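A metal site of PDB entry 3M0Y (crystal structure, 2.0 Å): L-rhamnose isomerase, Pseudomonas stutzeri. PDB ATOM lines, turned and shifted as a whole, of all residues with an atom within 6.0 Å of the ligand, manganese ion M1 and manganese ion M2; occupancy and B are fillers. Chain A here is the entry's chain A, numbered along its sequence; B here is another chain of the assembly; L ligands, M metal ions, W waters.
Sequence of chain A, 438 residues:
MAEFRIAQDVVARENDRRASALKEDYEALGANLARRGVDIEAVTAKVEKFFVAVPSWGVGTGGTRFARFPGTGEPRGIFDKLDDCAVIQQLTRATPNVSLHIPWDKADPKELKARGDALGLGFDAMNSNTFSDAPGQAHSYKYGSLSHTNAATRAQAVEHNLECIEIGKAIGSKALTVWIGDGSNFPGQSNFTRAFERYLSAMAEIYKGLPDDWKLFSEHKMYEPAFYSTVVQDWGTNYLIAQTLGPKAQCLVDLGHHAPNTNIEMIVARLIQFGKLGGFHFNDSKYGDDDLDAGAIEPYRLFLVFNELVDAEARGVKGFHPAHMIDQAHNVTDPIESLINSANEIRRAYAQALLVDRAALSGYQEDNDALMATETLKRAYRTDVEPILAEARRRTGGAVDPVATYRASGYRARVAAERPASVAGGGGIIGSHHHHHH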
ATOM      1  N   TRP A  57       8.138  22.767   9.795  1.00  0.00           N
ATOM      2  CA  TRP A  57       7.301  21.651  10.215  1.00  0.00           C
ATOM      3  C   TRP A  57       6.053  21.393   9.362  1.00  0.00           C
ATOM      4  O   TRP A  57       5.314  20.438   9.599  1.00  0.00           O
ATOM      5  CB  TRP A  57       6.909  21.824  11.685  1.00  0.00           C
ATOM      6  CG  TRP A  57       6.078  23.055  11.983  1.00  0.00           C
ATOM      7  CD1 TRP A  57       4.718  23.165  11.948  1.00  0.00           C
ATOM      8  CD2 TRP A  57       6.569  24.350  12.368  1.00  0.00           C
ATOM      9  NE1 TRP A  57       4.330  24.438  12.277  1.00  0.00           N
ATOM     10  CE2 TRP A  57       5.437  25.188  12.542  1.00  0.00           C
ATOM     11  CE3 TRP A  57       7.845  24.889  12.570  1.00  0.00           C
ATOM     12  CZ2 TRP A  57       5.556  26.532  12.912  1.00  0.00           C
ATOM     13  CZ3 TRP A  57       7.965  26.222  12.941  1.00  0.00           C
ATOM     14  CH2 TRP A  57       6.816  27.029  13.115  1.00  0.00           C
ATOM     15  N   HIS A 101      12.065  24.977  14.110  1.00  0.00           N
ATOM     16  CA  HIS A 101      11.556  24.432  15.357  1.00  0.00           C
ATOM     17  C   HIS A 101      12.628  23.563  16.005  1.00  0.00           C
ATOM     18  O   HIS A 101      13.171  22.665  15.366  1.00  0.00           O
ATOM     19  CB  HIS A 101      10.299  23.592  15.078  1.00  0.00           C
ATOM     20  CG  HIS A 101       9.214  23.767  16.102  1.00  0.00           C
ATOM     21  ND1 HIS A 101       9.395  23.470  17.441  1.00  0.00           N
ATOM     22  CD2 HIS A 101       7.952  24.254  15.993  1.00  0.00           C
ATOM     23  CE1 HIS A 101       8.290  23.762  18.100  1.00  0.00           C
ATOM     24  NE2 HIS A 101       7.395  24.231  17.249  1.00  0.00           N
ATOM     25  N   TRP A 104      13.406  19.680  16.707  1.00  0.00           N
ATOM     26  CA  TRP A 104      13.141  19.052  15.420  1.00  0.00           C
ATOM     27  C   TRP A 104      14.179  19.372  14.343  1.00  0.00           C
ATOM     28  O   TRP A 104      14.680  18.474  13.659  1.00  0.00           O
ATOM     29  CB  TRP A 104      11.761  19.453  14.876  1.00  0.00           C
ATOM     30  CG  TRP A 104      10.600  18.946  15.682  1.00  0.00           C
ATOM     31  CD1 TRP A 104      10.601  17.884  16.547  1.00  0.00           C
ATOM     32  CD2 TRP A 104       9.261  19.456  15.665  1.00  0.00           C
ATOM     33  NE1 TRP A 104       9.343  17.706  17.062  1.00  0.00           N
ATOM     34  CE2 TRP A 104       8.502  18.656  16.544  1.00  0.00           C
ATOM     35  CE3 TRP A 104       8.634  20.512  14.994  1.00  0.00           C
ATOM     36  CZ2 TRP A 104       7.135  18.868  16.770  1.00  0.00           C
ATOM     37  CZ3 TRP A 104       7.273  20.733  15.211  1.00  0.00           C
ATOM     38  CH2 TRP A 104       6.538  19.907  16.097  1.00  0.00           C
ATOM     39  N   ASN A 127      11.412  28.740  17.133  1.00  0.00           N
ATOM     40  CA  ASN A 127      10.289  28.188  17.869  1.00  0.00           C
ATOM     41  C   ASN A 127      10.803  27.145  18.846  1.00  0.00           C
ATOM     42  O   ASN A 127      11.465  26.197  18.444  1.00  0.00           O
ATOM     43  CB  ASN A 127       9.281  27.528  16.914  1.00  0.00           C
ATOM     44  CG  ASN A 127       8.582  28.520  16.022  1.00  0.00           C
ATOM     45  OD1 ASN A 127       7.515  29.041  16.360  1.00  0.00           O
ATOM     46  ND2 ASN A 127       9.164  28.791  14.867  1.00  0.00           N
ATOM     47  N   SER A 128      10.487  27.323  20.121  1.00  0.00           N
ATOM     48  CA  SER A 128      10.912  26.366  21.139  1.00  0.00           C
ATOM     49  C   SER A 128       9.880  25.243  21.251  1.00  0.00           C
ATOM     50  O   SER A 128       8.714  25.414  20.871  1.00  0.00           O
ATOM     51  CB  SER A 128      11.079  27.051  22.487  1.00  0.00           C
ATOM     52  OG  SER A 128       9.868  27.665  22.886  1.00  0.00           O
ATOM     53  N   PHE A 131       6.578  21.073  24.665  1.00  0.00           N
ATOM     54  CA  PHE A 131       5.264  20.455  24.678  1.00  0.00           C
ATOM     55  C   PHE A 131       5.383  18.957  24.324  1.00  0.00           C
ATOM     56  O   PHE A 131       4.388  18.257  24.132  1.00  0.00           O
ATOM     57  CB  PHE A 131       4.304  21.178  23.729  1.00  0.00           C
ATOM     58  CG  PHE A 131       4.785  21.265  22.308  1.00  0.00           C
ATOM     59  CD1 PHE A 131       4.774  20.142  21.481  1.00  0.00           C
ATOM     60  CD2 PHE A 131       5.279  22.473  21.793  1.00  0.00           C
ATOM     61  CE1 PHE A 131       5.234  20.209  20.172  1.00  0.00           C
ATOM     62  CE2 PHE A 131       5.738  22.550  20.483  1.00  0.00           C
ATOM     63  CZ  PHE A 131       5.715  21.428  19.671  1.00  0.00           C
ATOM     64  N   THR A 177       9.620  32.445  19.359  1.00  0.00           N
ATOM     65  CA  THR A 177       8.189  32.263  19.572  1.00  0.00           C
ATOM     66  C   THR A 177       8.006  31.160  20.598  1.00  0.00           C
ATOM     67  O   THR A 177       8.579  30.072  20.461  1.00  0.00           O
ATOM     68  CB  THR A 177       7.466  31.858  18.285  1.00  0.00           C
ATOM     69  OG1 THR A 177       7.504  32.958  17.361  1.00  0.00           O
ATOM     70  CG2 THR A 177       6.005  31.489  18.569  1.00  0.00           C
ATOM     71  N   TRP A 179       5.232  28.810  22.394  1.00  0.00           N
ATOM     72  CA  TRP A 179       3.907  28.235  22.525  1.00  0.00           C
ATOM     73  C   TRP A 179       4.098  26.974  23.329  1.00  0.00           C
ATOM     74  O   TRP A 179       4.964  26.158  22.995  1.00  0.00           O
ATOM     75  CB  TRP A 179       3.289  27.855  21.180  1.00  0.00           C
ATOM     76  CG  TRP A 179       2.004  27.110  21.386  1.00  0.00           C
ATOM     77  CD1 TRP A 179       0.801  27.633  21.782  1.00  0.00           C
ATOM     78  CD2 TRP A 179       1.816  25.684  21.321  1.00  0.00           C
ATOM     79  NE1 TRP A 179      -0.116  26.625  21.981  1.00  0.00           N
ATOM     80  CE2 TRP A 179       0.478  25.420  21.699  1.00  0.00           C
ATOM     81  CE3 TRP A 179       2.649  24.611  20.981  1.00  0.00           C
ATOM     82  CZ2 TRP A 179      -0.036  24.125  21.755  1.00  0.00           C
ATOM     83  CZ3 TRP A 179       2.126  23.323  21.030  1.00  0.00           C
ATOM     84  CH2 TRP A 179       0.792  23.090  21.410  1.00  0.00           C
ATOM     85  N   GLU A 219       2.468  32.896  22.332  1.00  0.00           N
ATOM     86  CA  GLU A 219       1.301  32.494  21.561  1.00  0.00           C
ATOM     87  C   GLU A 219       0.181  31.894  22.404  1.00  0.00           C
ATOM     88  O   GLU A 219       0.351  30.853  23.031  1.00  0.00           O
ATOM     89  CB  GLU A 219       1.741  31.493  20.488  1.00  0.00           C
ATOM     90  CG  GLU A 219       0.616  30.887  19.668  1.00  0.00           C
ATOM     91  CD  GLU A 219       1.124  30.056  18.514  1.00  0.00           C
ATOM     92  OE1 GLU A 219       2.318  29.690  18.515  1.00  0.00           O
ATOM     93  OE2 GLU A 219       0.331  29.749  17.603  1.00  0.00           O
ATOM     94  N   LYS A 221      -3.578  30.117  23.109  1.00  0.00           N
ATOM     95  CA  LYS A 221      -4.392  29.074  22.497  1.00  0.00           C
ATOM     96  C   LYS A 221      -5.474  28.658  23.491  1.00  0.00           C
ATOM     97  O   LYS A 221      -5.185  28.320  24.637  1.00  0.00           O
ATOM     98  CB  LYS A 221      -3.530  27.867  22.121  1.00  0.00           C
ATOM     99  CG  LYS A 221      -4.261  26.861  21.230  1.00  0.00           C
ATOM    100  CD  LYS A 221      -3.365  25.690  20.867  1.00  0.00           C
ATOM    101  CE  LYS A 221      -4.052  24.731  19.908  1.00  0.00           C
ATOM    102  NZ  LYS A 221      -3.214  23.523  19.628  1.00  0.00           N
ATOM    103  N   GLU A 224      -6.186  22.480  23.650  1.00  0.00           N
ATOM    104  CA  GLU A 224      -5.389  21.487  22.909  1.00  0.00           C
ATOM    105  C   GLU A 224      -3.917  21.874  23.016  1.00  0.00           C
ATOM    106  O   GLU A 224      -3.501  22.899  22.483  1.00  0.00           O
ATOM    107  CB  GLU A 224      -5.774  21.399  21.421  1.00  0.00           C
ATOM    108  CG  GLU A 224      -4.959  20.308  20.698  1.00  0.00           C
ATOM    109  CD  GLU A 224      -5.090  20.306  19.177  1.00  0.00           C
ATOM    110  OE1 GLU A 224      -5.070  21.389  18.559  1.00  0.00           O
ATOM    111  OE2 GLU A 224      -5.186  19.203  18.601  1.00  0.00           O
ATOM    112  N   LEU A 252       1.610  36.866  19.790  1.00  0.00           N
ATOM    113  CA  LEU A 252       1.488  36.280  18.474  1.00  0.00           C
ATOM    114  C   LEU A 252       0.064  35.746  18.360  1.00  0.00           C
ATOM    115  O   LEU A 252      -0.417  35.028  19.240  1.00  0.00           O
ATOM    116  CB  LEU A 252       2.515  35.166  18.290  1.00  0.00           C
ATOM    117  CG  LEU A 252       2.569  34.568  16.885  1.00  0.00           C
ATOM    118  CD1 LEU A 252       4.014  34.260  16.534  1.00  0.00           C
ATOM    119  CD2 LEU A 252       1.690  33.329  16.816  1.00  0.00           C
ATOM    120  N   ASP A 254      -2.464  33.374  16.421  1.00  0.00           N
ATOM    121  CA  ASP A 254      -2.638  32.263  15.503  1.00  0.00           C
ATOM    122  C   ASP A 254      -4.156  32.212  15.285  1.00  0.00           C
ATOM    123  O   ASP A 254      -4.925  31.955  16.216  1.00  0.00           O
ATOM    124  CB  ASP A 254      -2.116  30.954  16.111  1.00  0.00           C
ATOM    125  CG  ASP A 254      -2.224  29.785  15.158  1.00  0.00           C
ATOM    126  OD1 ASP A 254      -1.262  28.995  15.039  1.00  0.00           O
ATOM    127  OD2 ASP A 254      -3.292  29.643  14.521  1.00  0.00           O
ATOM    128  N   HIS A 257      -6.698  29.672  16.965  1.00  0.00           N
ATOM    129  CA  HIS A 257      -6.619  29.458  18.412  1.00  0.00           C
ATOM    130  C   HIS A 257      -7.667  30.190  19.230  1.00  0.00           C
ATOM    131  O   HIS A 257      -7.454  30.416  20.425  1.00  0.00           O
ATOM    132  CB  HIS A 257      -5.242  29.883  18.927  1.00  0.00           C
ATOM    133  CG  HIS A 257      -4.125  28.991  18.488  1.00  0.00           C
ATOM    134  ND1 HIS A 257      -2.860  29.063  19.041  1.00  0.00           N
ATOM    135  CD2 HIS A 257      -4.069  28.015  17.556  1.00  0.00           C
ATOM    136  CE1 HIS A 257      -2.087  28.158  18.470  1.00  0.00           C
ATOM    137  NE2 HIS A 257      -2.795  27.508  17.573  1.00  0.00           N
ATOM    138  N   HIS A 281       0.207  33.843  12.882  1.00  0.00           N
ATOM    139  CA  HIS A 281       0.400  32.456  12.454  1.00  0.00           C
ATOM    140  C   HIS A 281      -0.845  32.298  11.588  1.00  0.00           C
ATOM    141  O   HIS A 281      -1.964  32.214  12.083  1.00  0.00           O
ATOM    142  CB  HIS A 281       0.389  31.481  13.638  1.00  0.00           C
ATOM    143  CG  HIS A 281       1.752  31.145  14.153  1.00  0.00           C
ATOM    144  ND1 HIS A 281       1.976  30.134  15.065  1.00  0.00           N
ATOM    145  CD2 HIS A 281       2.970  31.671  13.876  1.00  0.00           C
ATOM    146  CE1 HIS A 281       3.268  30.053  15.325  1.00  0.00           C
ATOM    147  NE2 HIS A 281       3.888  30.980  14.625  1.00  0.00           N
ATOM    148  N   ASN A 283      -3.461  30.569   8.922  1.00  0.00           N
ATOM    149  CA  ASN A 283      -4.059  29.279   8.591  1.00  0.00           C
ATOM    150  C   ASN A 283      -5.564  29.508   8.579  1.00  0.00           C
ATOM    151  O   ASN A 283      -6.022  30.629   8.806  1.00  0.00           O
ATOM    152  CB  ASN A 283      -3.664  28.221   9.640  1.00  0.00           C
ATOM    153  CG  ASN A 283      -3.930  28.665  11.061  1.00  0.00           C
ATOM    154  OD1 ASN A 283      -5.058  28.971  11.434  1.00  0.00           O
ATOM    155  ND2 ASN A 283      -2.873  28.695  11.872  1.00  0.00           N
ATOM    156  N   ASP A 289      -8.584  24.240  16.131  1.00  0.00           N
ATOM    157  CA  ASP A 289      -7.315  24.665  15.553  1.00  0.00           C
ATOM    158  C   ASP A 289      -7.020  23.691  14.414  1.00  0.00           C
ATOM    159  O   ASP A 289      -6.084  22.879  14.480  1.00  0.00           O
ATOM    160  CB  ASP A 289      -6.220  24.639  16.625  1.00  0.00           C
ATOM    161  CG  ASP A 289      -4.867  25.068  16.087  1.00  0.00           C
ATOM    162  OD1 ASP A 289      -4.826  25.926  15.173  1.00  0.00           O
ATOM    163  OD2 ASP A 289      -3.847  24.561  16.592  1.00  0.00           O
ATOM    164  N   ASP A 291      -5.778  24.143  11.453  1.00  0.00           N
ATOM    165  CA  ASP A 291      -4.545  24.352  10.713  1.00  0.00           C
ATOM    166  C   ASP A 291      -4.637  24.102   9.206  1.00  0.00           C
ATOM    167  O   ASP A 291      -3.715  23.544   8.602  1.00  0.00           O
ATOM    168  CB  ASP A 291      -3.435  23.460  11.302  1.00  0.00           C
ATOM    169  CG  ASP A 291      -2.886  23.990  12.613  1.00  0.00           C
ATOM    170  OD1 ASP A 291      -2.587  25.203  12.657  1.00  0.00           O
ATOM    171  OD2 ASP A 291      -2.741  23.210  13.582  1.00  0.00           O
ATOM    172  N   ASP A 327       1.400  28.825   9.790  1.00  0.00           N
ATOM    173  CA  ASP A 327       1.500  27.699  10.709  1.00  0.00           C
ATOM    174  C   ASP A 327       0.348  26.796  10.311  1.00  0.00           C
ATOM    175  O   ASP A 327      -0.779  26.970  10.766  1.00  0.00           O
ATOM    176  CB  ASP A 327       1.333  28.128  12.171  1.00  0.00           C
ATOM    177  CG  ASP A 327       1.424  26.948  13.148  1.00  0.00           C
ATOM    178  OD1 ASP A 327       1.674  25.805  12.682  1.00  0.00           O
ATOM    179  OD2 ASP A 327       1.247  27.165  14.367  1.00  0.00           O
ATOM    180  N   ARG B  65      -2.109  15.079  19.077  1.00  0.00           N
ATOM    181  CA  ARG B  65      -1.247  15.166  17.907  1.00  0.00           C
ATOM    182  C   ARG B  65       0.106  15.772  18.257  1.00  0.00           C
ATOM    183  O   ARG B  65       1.072  15.627  17.508  1.00  0.00           O
ATOM    184  CB  ARG B  65      -1.906  15.997  16.810  1.00  0.00           C
ATOM    185  CG  ARG B  65      -2.256  17.413  17.202  1.00  0.00           C
ATOM    186  CD  ARG B  65      -2.861  18.169  16.022  1.00  0.00           C
ATOM    187  NE  ARG B  65      -3.365  19.478  16.423  1.00  0.00           N
ATOM    188  CZ  ARG B  65      -3.342  20.564  15.654  1.00  0.00           C
ATOM    189  NH1 ARG B  65      -2.821  20.497  14.435  1.00  0.00           N
ATOM    190  NH2 ARG B  65      -3.816  21.711  16.109  1.00  0.00           N
ATOM    191  N   PHE B  66       0.197  16.454  19.392  1.00  0.00           N
ATOM    192  CA  PHE B  66       1.443  17.076  19.809  1.00  0.00           C
ATOM    193  C   PHE B  66       2.365  16.156  20.595  1.00  0.00           C
ATOM    194  O   PHE B  66       3.587  16.257  20.488  1.00  0.00           O
ATOM    195  CB  PHE B  66       1.153  18.336  20.624  1.00  0.00           C
ATOM    196  CG  PHE B  66       0.527  19.429  19.826  1.00  0.00           C
ATOM    197  CD1 PHE B  66       1.289  20.175  18.925  1.00  0.00           C
ATOM    198  CD2 PHE B  66      -0.829  19.699  19.942  1.00  0.00           C
ATOM    199  CE1 PHE B  66       0.705  21.163  18.150  1.00  0.00           C
ATOM    200  CE2 PHE B  66      -1.428  20.696  19.168  1.00  0.00           C
ATOM    201  CZ  PHE B  66      -0.650  21.424  18.268  1.00  0.00           C
HETATM  202  C1  LIG L   1       0.126  24.970  18.411  1.00  0.00           C
HETATM  203  C2  LIG L   1       0.665  26.283  17.877  1.00  0.00           C
HETATM  204  C3  LIG L   1       2.182  26.215  17.702  1.00  0.00           C
HETATM  205  C4  LIG L   1       2.599  24.913  17.015  1.00  0.00           C
HETATM  206  C5  LIG L   1       4.044  24.986  16.549  1.00  0.00           C
HETATM  207  C6  LIG L   1       4.426  23.679  15.860  1.00  0.00           C
HETATM  208  O1  LIG L   1      -1.092  24.756  18.411  1.00  0.00           O
HETATM  209  O2  LIG L   1       0.059  26.573  16.622  1.00  0.00           O
HETATM  210  O3  LIG L   1       2.627  27.319  16.947  1.00  0.00           O
HETATM  211  O4  LIG L   1       1.753  24.667  15.894  1.00  0.00           O
HETATM  212  O5  LIG L   1       4.900  25.202  17.667  1.00  0.00           O
HETATM  213 MN    MN M   1       0.713  28.537  15.839  1.00  0.00          MN
HETATM  214 MN    MN M   2      -2.022  25.652  16.675  1.00  0.00          MN
HETATM  215  O   HOH W   1      -2.370  26.353  14.706  1.00  0.00           O
HETATM  216  O   HOH W   2       5.601  27.702  18.193  1.00  0.00           O
HETATM  217  O   HOH W   3      -1.213  23.935  15.547  1.00  0.00           O
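A ring nitrogen (NE2) of His 101 sits at hydrogen-bond distance from an oxygen (O5) of the ligand, at 2.7 Å. The side-chain amino group (NZ) of Lys 221 lies close to an oxygen (O1) of the ligand (2.7 Å).
The backbone carbonyl oxygen of Asp 327 sits at hydrogen-bond distance from the side-chain amide nitrogen of Asn 283 (2.9 Å). NZ of Lys 221 is in salt-bridge range of OE1 of Glu 224 (3.0 Å). The indole nitrogen of Trp 57 lies within hydrogen-bond range of the side-chain carboxylate of Asp 327. OD2 of Asp 289 sits close to NZ of Lys 221, 3.3 Å away. The side-chain carboxylate (OD2) of Asp 254 sits at hydrogen-bond distance from the side-chain amide nitrogen (ND2) of Asn 283, at 2.8 Å. NH2 of Arg 65 of chain B is in hydrogen-bond range of O of Asp 289 (3.0 Å).
Merely in contact with the ligand: Trp 179 (3.3 Å), Phe 66 of chain B (3.4 Å), Trp 57 (3.7 Å) and Phe 131 (3.96 Å). Hydrophobic or aromatic side chains that line the ligand: Trp 57, His 101, Phe 131, Trp 179, His 257, His 281 and Phe 66 of chain B. 12 residues have an atom within 4 Å of the ligand: Trp 57, His 101, Phe 131, Trp 179, Glu 219, Lys 221, Asp 254, His 257, His 281, Asp 289, Asp 327 and Phe 66 of chain B. The nearest printed residue that does not touch the ligand is Trp 104 (4.1 Å).
The nearest printed residue that does not touch manganese ion M1 is Leu 252 (5.0 Å).
Lys 221 touches manganese ion M2 (NZ to MN, 3.8 Å). Of the 21 residues printed, 4 come within 4 Å of manganese ion M2. The nearest printed residue that does not touch manganese ion M2 is Asp 291 (4.01 Å).
Manganese ion M1 is bound by OD2 of Asp 327 (2.1 Å), OE2 of Glu 219 (2.2 Å), ND1 of His 281 (2.2 Å), OD1 of Asp 254 (2.2 Å), O2 of the ligand (2.2 Å) and O3 of the ligand (2.5 Å).
Manganese ion M2 is bound by water W1, 2.1 Å away. The side-chain carboxylate (OD2) of Asp 289 binds manganese ion M2, 2.1 Å away. O1 of the ligand is bound to manganese ion M2, 2.2 Å away. NE2 of His 257 is bound to manganese ion M2 (2.2 Å). Water W3 binds manganese ion M2, at 2.2 Å. An oxygen (O2) of the ligand binds manganese ion M2.
Water W3 lies within hydrogen-bond range of OD2 of Asp 291 (2.6 Å), O4 of the ligand (3.1 Å) and NH2 of Arg 65 of chain B (3.5 Å). Water W2 lies within hydrogen-bond range of an oxygen (O5) of the ligand (2.6 Å) and the side-chain amide oxygen (OD1) of Asn 127 (3.0 Å).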
